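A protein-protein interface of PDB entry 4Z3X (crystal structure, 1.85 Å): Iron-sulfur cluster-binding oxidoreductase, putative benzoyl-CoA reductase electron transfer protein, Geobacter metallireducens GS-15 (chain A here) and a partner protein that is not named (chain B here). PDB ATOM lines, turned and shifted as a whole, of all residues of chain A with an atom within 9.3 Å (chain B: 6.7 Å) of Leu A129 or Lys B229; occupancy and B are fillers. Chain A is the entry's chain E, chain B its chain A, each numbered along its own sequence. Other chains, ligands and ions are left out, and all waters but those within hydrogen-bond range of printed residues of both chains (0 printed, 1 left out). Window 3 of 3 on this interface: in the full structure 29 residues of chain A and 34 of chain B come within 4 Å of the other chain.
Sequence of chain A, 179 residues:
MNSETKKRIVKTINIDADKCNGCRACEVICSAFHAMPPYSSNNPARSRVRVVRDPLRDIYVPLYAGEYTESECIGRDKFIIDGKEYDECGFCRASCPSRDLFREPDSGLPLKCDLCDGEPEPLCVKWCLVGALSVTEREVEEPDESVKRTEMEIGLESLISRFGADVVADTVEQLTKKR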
ATOM      1  N   LYS A  19     -25.862  27.594  -1.936  1.00  0.00           N
ATOM      2  CA  LYS A  19     -24.959  26.483  -1.929  1.00  0.00           C
ATOM      3  C   LYS A  19     -25.256  25.601  -0.684  1.00  0.00           C
ATOM      4  O   LYS A  19     -24.690  24.496  -0.551  1.00  0.00           O
ATOM      5  CB  LYS A  19     -23.502  26.976  -1.935  1.00  0.00           C
ATOM      6  CG  LYS A  19     -22.873  27.309  -3.260  1.00  0.00           C
ATOM      7  CD  LYS A  19     -21.446  27.768  -2.927  1.00  0.00           C
ATOM      8  CE  LYS A  19     -20.488  27.749  -4.072  1.00  0.00           C
ATOM      9  NZ  LYS A  19     -19.098  27.941  -3.479  1.00  0.00           N
ATOM     10  N   ASN A  21     -26.722  22.883   1.828  1.00  0.00           N
ATOM     11  CA  ASN A  21     -27.451  21.579   1.628  1.00  0.00           C
ATOM     12  C   ASN A  21     -28.202  21.178   2.881  1.00  0.00           C
ATOM     13  O   ASN A  21     -28.738  20.068   2.942  1.00  0.00           O
ATOM     14  CB  ASN A  21     -26.511  20.401   1.243  1.00  0.00           C
ATOM     15  CG  ASN A  21     -25.364  20.244   2.212  1.00  0.00           C
ATOM     16  OD1 ASN A  21     -25.568  20.188   3.404  1.00  0.00           O
ATOM     17  ND2 ASN A  21     -24.137  20.208   1.705  1.00  0.00           N
ATOM     18  N   CYS A  23     -27.166  20.493   6.070  1.00  0.00           N
ATOM     19  CA  CYS A  23     -26.596  19.299   6.744  1.00  0.00           C
ATOM     20  C   CYS A  23     -26.458  19.580   8.221  1.00  0.00           C
ATOM     21  O   CYS A  23     -26.463  18.664   9.055  1.00  0.00           O
ATOM     22  CB  CYS A  23     -25.244  18.925   6.165  1.00  0.00           C
ATOM     23  SG  CYS A  23     -23.927  20.069   6.411  1.00  0.00           S
ATOM     24  N   ALA A  25     -23.838  20.752   9.687  1.00  0.00           N
ATOM     25  CA  ALA A  25     -22.479  20.405  10.172  1.00  0.00           C
ATOM     26  C   ALA A  25     -21.876  21.569  10.991  1.00  0.00           C
ATOM     27  O   ALA A  25     -21.079  21.429  11.949  1.00  0.00           O
ATOM     28  CB  ALA A  25     -21.506  20.027   8.894  1.00  0.00           C
ATOM     29  N   CYS A  26     -22.239  22.763  10.582  1.00  0.00           N
ATOM     30  CA  CYS A  26     -21.848  23.981  11.245  1.00  0.00           C
ATOM     31  C   CYS A  26     -22.338  24.065  12.691  1.00  0.00           C
ATOM     32  O   CYS A  26     -21.553  24.417  13.612  1.00  0.00           O
ATOM     33  CB  CYS A  26     -22.349  25.152  10.385  1.00  0.00           C
ATOM     34  SG  CYS A  26     -24.109  25.105   9.794  1.00  0.00           S
ATOM     35  N   GLU A 121      -8.978  29.514  12.252  1.00  0.00           N
ATOM     36  CA  GLU A 121     -10.072  29.761  11.302  1.00  0.00           C
ATOM     37  C   GLU A 121     -11.449  29.383  11.919  1.00  0.00           C
ATOM     38  O   GLU A 121     -11.549  28.478  12.764  1.00  0.00           O
ATOM     39  CB  GLU A 121      -9.754  28.992   9.999  1.00  0.00           C
ATOM     40  CG  GLU A 121     -10.879  28.650   8.994  1.00  0.00           C
ATOM     41  CD  GLU A 121     -10.506  27.423   8.067  1.00  0.00           C
ATOM     42  OE1 GLU A 121      -9.623  26.614   8.453  1.00  0.00           O
ATOM     43  OE2 GLU A 121     -11.105  27.254   6.967  1.00  0.00           O
ATOM     44  N   LEU A 123     -14.607  27.542  12.693  1.00  0.00           N
ATOM     45  CA  LEU A 123     -14.809  26.075  12.599  1.00  0.00           C
ATOM     46  C   LEU A 123     -16.005  25.720  11.726  1.00  0.00           C
ATOM     47  O   LEU A 123     -15.972  24.722  11.001  1.00  0.00           O
ATOM     48  CB  LEU A 123     -14.943  25.487  14.016  1.00  0.00           C
ATOM     49  CG  LEU A 123     -13.502  25.477  14.579  1.00  0.00           C
ATOM     50  CD1 LEU A 123     -13.461  25.622  16.063  1.00  0.00           C
ATOM     51  CD2 LEU A 123     -12.738  24.224  14.149  1.00  0.00           C
ATOM     52  N   CYS A 124     -17.051  26.549  11.751  1.00  0.00           N
ATOM     53  CA  CYS A 124     -18.219  26.323  10.874  1.00  0.00           C
ATOM     54  C   CYS A 124     -17.783  26.457   9.395  1.00  0.00           C
ATOM     55  O   CYS A 124     -18.117  25.601   8.575  1.00  0.00           O
ATOM     56  CB  CYS A 124     -19.353  27.314  11.220  1.00  0.00           C
ATOM     57  SG  CYS A 124     -18.798  29.111  11.084  1.00  0.00           S
ATOM     58  N   VAL A 125     -17.001  27.493   9.050  1.00  0.00           N
ATOM     59  CA  VAL A 125     -16.435  27.572   7.702  1.00  0.00           C
ATOM     60  C   VAL A 125     -15.553  26.335   7.327  1.00  0.00           C
ATOM     61  O   VAL A 125     -15.686  25.819   6.201  1.00  0.00           O
ATOM     62  CB  VAL A 125     -15.635  28.878   7.521  1.00  0.00           C
ATOM     63  CG1 VAL A 125     -15.029  28.996   6.138  1.00  0.00           C
ATOM     64  CG2 VAL A 125     -16.552  30.033   7.769  1.00  0.00           C
ATOM     65  N   LYS A 126     -14.658  25.887   8.220  1.00  0.00           N
ATOM     66  CA  LYS A 126     -13.852  24.662   7.980  1.00  0.00           C
ATOM     67  C   LYS A 126     -14.680  23.408   7.684  1.00  0.00           C
ATOM     68  O   LYS A 126     -14.287  22.571   6.835  1.00  0.00           O
ATOM     69  CB  LYS A 126     -12.941  24.392   9.184  1.00  0.00           C
ATOM     70  CG  LYS A 126     -11.924  23.337   8.903  1.00  0.00           C
ATOM     71  CD  LYS A 126     -10.846  23.182   9.994  1.00  0.00           C
ATOM     72  CE  LYS A 126     -11.321  22.307  11.141  1.00  0.00           C
ATOM     73  NZ  LYS A 126     -10.173  21.832  11.963  1.00  0.00           N
ATOM     74  N   TRP A 127     -15.822  23.237   8.365  1.00  0.00           N
ATOM     75  CA  TRP A 127     -16.534  21.967   8.286  1.00  0.00           C
ATOM     76  C   TRP A 127     -17.585  22.054   7.198  1.00  0.00           C
ATOM     77  O   TRP A 127     -18.202  21.053   6.895  1.00  0.00           O
ATOM     78  CB  TRP A 127     -17.212  21.604   9.628  1.00  0.00           C
ATOM     79  CG  TRP A 127     -16.289  20.842  10.506  1.00  0.00           C
ATOM     80  CD1 TRP A 127     -14.967  21.099  10.690  1.00  0.00           C
ATOM     81  CD2 TRP A 127     -16.596  19.668  11.297  1.00  0.00           C
ATOM     82  NE1 TRP A 127     -14.441  20.187  11.572  1.00  0.00           N
ATOM     83  CE2 TRP A 127     -15.409  19.287  11.945  1.00  0.00           C
ATOM     84  CE3 TRP A 127     -17.773  18.939  11.555  1.00  0.00           C
ATOM     85  CZ2 TRP A 127     -15.331  18.163  12.809  1.00  0.00           C
ATOM     86  CZ3 TRP A 127     -17.700  17.805  12.401  1.00  0.00           C
ATOM     87  CH2 TRP A 127     -16.475  17.441  13.024  1.00  0.00           C
ATOM     88  N   CYS A 128     -17.818  23.260   6.642  1.00  0.00           N
ATOM     89  CA  CYS A 128     -18.721  23.392   5.479  1.00  0.00           C
ATOM     90  C   CYS A 128     -17.944  22.935   4.236  1.00  0.00           C
ATOM     91  O   CYS A 128     -17.417  23.769   3.487  1.00  0.00           O
ATOM     92  CB  CYS A 128     -19.224  24.846   5.261  1.00  0.00           C
ATOM     93  SG  CYS A 128     -20.606  24.867   4.045  1.00  0.00           S
ATOM     94  N   LEU A 129     -17.872  21.617   4.033  1.00  0.00           N
ATOM     95  CA  LEU A 129     -17.079  21.097   2.936  1.00  0.00           C
ATOM     96  C   LEU A 129     -17.621  21.607   1.591  1.00  0.00           C
ATOM     97  O   LEU A 129     -16.874  21.752   0.649  1.00  0.00           O
ATOM     98  CB  LEU A 129     -17.031  19.536   2.988  1.00  0.00           C
ATOM     99  CG  LEU A 129     -15.646  19.060   3.486  1.00  0.00           C
ATOM    100  CD1 LEU A 129     -15.241  19.720   4.836  1.00  0.00           C
ATOM    101  CD2 LEU A 129     -15.369  17.516   3.524  1.00  0.00           C
ATOM    102  N   VAL A 130     -18.898  21.965   1.499  1.00  0.00           N
ATOM    103  CA  VAL A 130     -19.394  22.468   0.212  1.00  0.00           C
ATOM    104  C   VAL A 130     -19.072  24.001   0.022  1.00  0.00           C
ATOM    105  O   VAL A 130     -19.261  24.530  -1.070  1.00  0.00           O
ATOM    106  CB  VAL A 130     -20.894  22.212   0.006  1.00  0.00           C
ATOM    107  CG1 VAL A 130     -21.189  20.654   0.140  1.00  0.00           C
ATOM    108  CG2 VAL A 130     -21.867  23.124   0.996  1.00  0.00           C
ATOM    109  N   GLY A 131     -18.522  24.670   1.036  1.00  0.00           N
ATOM    110  CA  GLY A 131     -18.014  26.029   0.832  1.00  0.00           C
ATOM    111  C   GLY A 131     -19.104  27.099   0.730  1.00  0.00           C
ATOM    112  O   GLY A 131     -19.015  28.019  -0.064  1.00  0.00           O
ATOM    113  N   ALA A 132     -20.155  26.963   1.515  1.00  0.00           N
ATOM    114  CA  ALA A 132     -21.266  27.910   1.552  1.00  0.00           C
ATOM    115  C   ALA A 132     -20.897  29.194   2.349  1.00  0.00           C
ATOM    116  O   ALA A 132     -21.590  30.182   2.313  1.00  0.00           O
ATOM    117  CB  ALA A 132     -22.552  27.237   2.203  1.00  0.00           C
ATOM    118  N   LEU A 133     -19.808  29.125   3.101  1.00  0.00           N
ATOM    119  CA  LEU A 133     -19.518  30.070   4.136  1.00  0.00           C
ATOM    120  C   LEU A 133     -18.088  30.516   4.006  1.00  0.00           C
ATOM    121  O   LEU A 133     -17.169  29.730   3.696  1.00  0.00           O
ATOM    122  CB  LEU A 133     -19.720  29.489   5.514  1.00  0.00           C
ATOM    123  CG  LEU A 133     -20.949  28.672   5.801  1.00  0.00           C
ATOM    124  CD1 LEU A 133     -20.651  27.954   7.121  1.00  0.00           C
ATOM    125  CD2 LEU A 133     -22.211  29.550   5.915  1.00  0.00           C
ATOM    126  N   THR B  73     -18.923  12.532  11.040  1.00  0.00           N
ATOM    127  CA  THR B  73     -19.571  12.810   9.756  1.00  0.00           C
ATOM    128  C   THR B  73     -20.498  11.695   9.294  1.00  0.00           C
ATOM    129  O   THR B  73     -20.118  10.504   9.307  1.00  0.00           O
ATOM    130  CB  THR B  73     -18.493  13.067   8.666  1.00  0.00           C
ATOM    131  OG1 THR B  73     -17.568  14.023   9.174  1.00  0.00           O
ATOM    132  CG2 THR B  73     -19.113  13.601   7.373  1.00  0.00           C
ATOM    133  N   ASN B 222     -11.800  14.827  11.837  1.00  0.00           N
ATOM    134  CA  ASN B 222     -11.137  15.742  10.903  1.00  0.00           C
ATOM    135  C   ASN B 222     -10.368  14.945   9.862  1.00  0.00           C
ATOM    136  O   ASN B 222     -10.322  15.294   8.677  1.00  0.00           O
ATOM    137  CB  ASN B 222     -10.205  16.706  11.658  1.00  0.00           C
ATOM    138  CG  ASN B 222     -10.972  17.868  12.245  1.00  0.00           C
ATOM    139  OD1 ASN B 222     -11.798  18.464  11.555  1.00  0.00           O
ATOM    140  ND2 ASN B 222     -10.760  18.156  13.523  1.00  0.00           N
ATOM    141  N   VAL B 224     -11.379  12.095   8.848  1.00  0.00           N
ATOM    142  CA  VAL B 224     -12.399  11.621   7.938  1.00  0.00           C
ATOM    143  C   VAL B 224     -12.714  12.701   6.878  1.00  0.00           C
ATOM    144  O   VAL B 224     -12.715  12.390   5.672  1.00  0.00           O
ATOM    145  CB  VAL B 224     -13.671  11.173   8.689  1.00  0.00           C
ATOM    146  CG1 VAL B 224     -14.888  11.228   7.774  1.00  0.00           C
ATOM    147  CG2 VAL B 224     -13.481   9.716   9.226  1.00  0.00           C
ATOM    148  N   LEU B 225     -12.966  13.949   7.314  1.00  0.00           N
ATOM    149  CA  LEU B 225     -13.220  15.058   6.401  1.00  0.00           C
ATOM    150  C   LEU B 225     -12.076  15.282   5.400  1.00  0.00           C
ATOM    151  O   LEU B 225     -12.321  15.485   4.211  1.00  0.00           O
ATOM    152  CB  LEU B 225     -13.490  16.363   7.192  1.00  0.00           C
ATOM    153  CG  LEU B 225     -14.801  16.432   8.016  1.00  0.00           C
ATOM    154  CD1 LEU B 225     -14.893  17.676   8.886  1.00  0.00           C
ATOM    155  CD2 LEU B 225     -16.078  16.296   7.127  1.00  0.00           C
ATOM    156  N   ASP B 226     -10.828  15.218   5.847  1.00  0.00           N
ATOM    157  CA  ASP B 226      -9.725  15.284   4.901  1.00  0.00           C
ATOM    158  C   ASP B 226      -9.760  14.127   3.889  1.00  0.00           C
ATOM    159  O   ASP B 226      -9.387  14.296   2.725  1.00  0.00           O
ATOM    160  CB  ASP B 226      -8.399  15.258   5.627  1.00  0.00           C
ATOM    161  CG  ASP B 226      -8.164  16.492   6.425  1.00  0.00           C
ATOM    162  OD1 ASP B 226      -8.835  17.525   6.151  1.00  0.00           O
ATOM    163  OD2 ASP B 226      -7.305  16.434   7.331  1.00  0.00           O
ATOM    164  N   TYR B 227     -10.203  12.958   4.325  1.00  0.00           N
ATOM    165  CA  TYR B 227     -10.159  11.817   3.420  1.00  0.00           C
ATOM    166  C   TYR B 227     -11.302  11.991   2.431  1.00  0.00           C
ATOM    167  O   TYR B 227     -11.152  11.711   1.244  1.00  0.00           O
ATOM    168  CB  TYR B 227     -10.266  10.477   4.164  1.00  0.00           C
ATOM    169  CG  TYR B 227     -10.002   9.298   3.248  1.00  0.00           C
ATOM    170  CD1 TYR B 227      -8.727   8.846   3.047  1.00  0.00           C
ATOM    171  CD2 TYR B 227     -11.015   8.729   2.528  1.00  0.00           C
ATOM    172  CE1 TYR B 227      -8.453   7.764   2.163  1.00  0.00           C
ATOM    173  CE2 TYR B 227     -10.769   7.654   1.636  1.00  0.00           C
ATOM    174  CZ  TYR B 227      -9.494   7.173   1.464  1.00  0.00           C
ATOM    175  OH  TYR B 227      -9.253   6.119   0.585  1.00  0.00           O
ATOM    176  N   ILE B 228     -12.434  12.500   2.902  1.00  0.00           N
ATOM    177  CA  ILE B 228     -13.543  12.759   1.977  1.00  0.00           C
ATOM    178  C   ILE B 228     -13.104  13.712   0.830  1.00  0.00           C
ATOM    179  O   ILE B 228     -13.425  13.474  -0.338  1.00  0.00           O
ATOM    180  CB  ILE B 228     -14.751  13.334   2.725  1.00  0.00           C
ATOM    181  CG1 ILE B 228     -15.427  12.212   3.568  1.00  0.00           C
ATOM    182  CG2 ILE B 228     -15.760  13.939   1.741  1.00  0.00           C
ATOM    183  CD1 ILE B 228     -16.547  12.703   4.511  1.00  0.00           C
ATOM    184  N   LYS B 229     -12.354  14.764   1.166  1.00  0.00           N
ATOM    185  CA  LYS B 229     -11.974  15.780   0.178  1.00  0.00           C
ATOM    186  C   LYS B 229     -11.114  15.123  -0.869  1.00  0.00           C
ATOM    187  O   LYS B 229     -11.275  15.321  -2.073  1.00  0.00           O
ATOM    188  CB  LYS B 229     -11.170  16.935   0.797  1.00  0.00           C
ATOM    189  CG  LYS B 229     -11.904  17.688   1.856  1.00  0.00           C
ATOM    190  CD  LYS B 229     -11.043  18.816   2.387  1.00  0.00           C
ATOM    191  CE  LYS B 229     -11.564  19.280   3.744  1.00  0.00           C
ATOM    192  NZ  LYS B 229     -10.753  20.487   4.181  1.00  0.00           N
ATOM    193  N   HIS B 230     -10.146  14.380  -0.374  1.00  0.00           N
ATOM    194  CA  HIS B 230      -9.173  13.748  -1.238  1.00  0.00           C
ATOM    195  C   HIS B 230      -9.789  12.672  -2.115  1.00  0.00           C
ATOM    196  O   HIS B 230      -9.435  12.544  -3.290  1.00  0.00           O
ATOM    197  CB  HIS B 230      -8.053  13.150  -0.412  1.00  0.00           C
ATOM    198  CG  HIS B 230      -7.077  12.367  -1.227  1.00  0.00           C
ATOM    199  ND1 HIS B 230      -7.080  10.988  -1.259  1.00  0.00           N
ATOM    200  CD2 HIS B 230      -6.087  12.765  -2.063  1.00  0.00           C
ATOM    201  CE1 HIS B 230      -6.128  10.568  -2.071  1.00  0.00           C
ATOM    202  NE2 HIS B 230      -5.513  11.624  -2.573  1.00  0.00           N
ATOM    203  N   ARG B 231     -10.706  11.902  -1.538  1.00  0.00           N
ATOM    204  CA  ARG B 231     -11.339  10.793  -2.228  1.00  0.00           C
ATOM    205  C   ARG B 231     -12.221  11.309  -3.363  1.00  0.00           C
ATOM    206  O   ARG B 231     -12.315  10.683  -4.429  1.00  0.00           O
ATOM    207  CB  ARG B 231     -12.163   9.951  -1.245  1.00  0.00           C
ATOM    208  CG  ARG B 231     -12.962   8.909  -1.850  1.00  0.00           C
ATOM    209  CD  ARG B 231     -12.111   7.704  -2.383  1.00  0.00           C
ATOM    210  NE  ARG B 231     -13.082   6.642  -2.665  1.00  0.00           N
ATOM    211  CZ  ARG B 231     -13.805   6.645  -3.771  1.00  0.00           C
ATOM    212  NH1 ARG B 231     -13.585   7.594  -4.690  1.00  0.00           N
ATOM    213  NH2 ARG B 231     -14.712   5.723  -3.969  1.00  0.00           N
ATOM    214  N   GLU B 232     -12.856  12.456  -3.141  1.00  0.00           N
ATOM    215  CA  GLU B 232     -13.748  13.021  -4.152  1.00  0.00           C
ATOM    216  C   GLU B 232     -12.941  13.695  -5.286  1.00  0.00           C
ATOM    217  O   GLU B 232     -13.477  13.935  -6.373  1.00  0.00           O
ATOM    218  CB  GLU B 232     -14.742  14.007  -3.515  1.00  0.00           C
ATOM    219  CG  GLU B 232     -15.913  13.301  -2.721  1.00  0.00           C
ATOM    220  CD  GLU B 232     -16.726  12.324  -3.604  1.00  0.00           C
ATOM    221  OE1 GLU B 232     -16.608  11.078  -3.427  1.00  0.00           O
ATOM    222  OE2 GLU B 232     -17.482  12.799  -4.491  1.00  0.00           O
ATOM    223  N   GLU B 233     -11.663  13.996  -5.031  1.00  0.00           N
ATOM    224  CA  GLU B 233     -10.744  14.449  -6.073  1.00  0.00           C
ATOM    225  C   GLU B 233     -10.183  13.267  -6.861  1.00  0.00           C
ATOM    226  O   GLU B 233      -9.458  13.461  -7.836  1.00  0.00           O
ATOM    227  CB  GLU B 233      -9.580  15.268  -5.482  1.00  0.00           C
ATOM    228  CG  GLU B 233     -10.021  16.567  -4.769  1.00  0.00           C
ATOM    229  CD  GLU B 233      -8.925  17.182  -3.894  1.00  0.00           C
ATOM    230  OE1 GLU B 233      -7.772  16.705  -3.953  1.00  0.00           O
ATOM    231  OE2 GLU B 233      -9.221  18.146  -3.144  1.00  0.00           O
ATOM    232  N   ASN B 234     -10.513  12.046  -6.431  1.00  0.00           N
ATOM    233  CA  ASN B 234      -9.942  10.838  -7.030  1.00  0.00           C
ATOM    234  C   ASN B 234     -10.947   9.727  -7.124  1.00  0.00           C
ATOM    235  O   ASN B 234     -10.856   8.751  -6.390  1.00  0.00           O
ATOM    236  CB  ASN B 234      -8.735  10.347  -6.228  1.00  0.00           C
ATOM    237  CG  ASN B 234      -7.581  11.328  -6.258  1.00  0.00           C
ATOM    238  OD1 ASN B 234      -6.703  11.234  -7.098  1.00  0.00           O
ATOM    239  ND2 ASN B 234      -7.590  12.289  -5.333  1.00  0.00           N
ATOM    240  N   LEU B 246     -17.906   8.565  -3.124  1.00  0.00           N
ATOM    241  CA  LEU B 246     -18.581   8.293  -1.850  1.00  0.00           C
ATOM    242  C   LEU B 246     -20.094   8.569  -1.911  1.00  0.00           C
ATOM    243  O   LEU B 246     -20.603   9.183  -2.853  1.00  0.00           O
ATOM    244  CB  LEU B 246     -17.919   9.110  -0.730  1.00  0.00           C
ATOM    245  CG  LEU B 246     -16.420   8.856  -0.528  1.00  0.00           C
ATOM    246  CD1 LEU B 246     -15.839   9.729   0.604  1.00  0.00           C
ATOM    247  CD2 LEU B 246     -16.211   7.357  -0.219  1.00  0.00           C
ATOM    248  N   PRO B 303     -21.473  16.077   4.004  1.00  0.00           N
ATOM    249  CA  PRO B 303     -21.363  16.953   2.823  1.00  0.00           C
ATOM    250  C   PRO B 303     -21.776  16.326   1.497  1.00  0.00           C
ATOM    251  O   PRO B 303     -21.876  17.042   0.496  1.00  0.00           O
ATOM    252  CB  PRO B 303     -19.876  17.299   2.813  1.00  0.00           C
ATOM    253  CG  PRO B 303     -19.233  15.978   3.261  1.00  0.00           C
ATOM    254  CD  PRO B 303     -20.149  15.618   4.453  1.00  0.00           C
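Of the 17 printed residues of chain A, 4 touch a printed residue of chain B. Printed residues of chain A that touch a printed residue of chain B: Lys A126, Trp A127, Leu A129 and Val A130. Hydrophobic or aromatic side chains of chain A that line the printed part of chain B: Trp A127, Leu A129 and Val A130. Of the 15 printed residues of chain B, 4 touch a printed residue of chain A. Printed residues of chain B that touch a printed residue of chain A: Asn B222, Leu B225, Lys B229 and Pro B303.
Asn B222 touches Lys A126. Trp A127 touches Leu B225 (CE2 to CD1, 3.5 Å). O of Leu B225 touches CD2 of Leu A129, at 3.7 Å. Leu A129 touches Lys B229. Pro B303 touches Leu A129. Val A130 touches Pro B303.
Printed residues of chain B within 4 Å of Leu A129: Leu B225 (3.7 Å), Lys B229 (3.8 Å) and Pro B303 (3.6 Å). Printed residues of chain B within 4 Å of Trp A127: Asn B222 (3.2 Å) and Leu B225 (3.5 Å). Printed residues of chain A within 4 Å of Leu B225: Trp A127 and Leu A129. Of the printed residues of chain B, Val A130 touches Pro B303 (3.7 Å). Printed residues of chain A within 4 Å of Pro B303: Leu A129 and Val A130. Printed residues of chain B within 4 Å of Lys A126: Asn B222. The nearest printed residue of chain B that does not touch Leu A129 is Ile B228 (4.02 Å).
The side-chain amide oxygen (OD1) of Asn B222 is in hydrogen-bond range of the indole nitrogen (NE1) of Trp A127 (3.2 Å).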
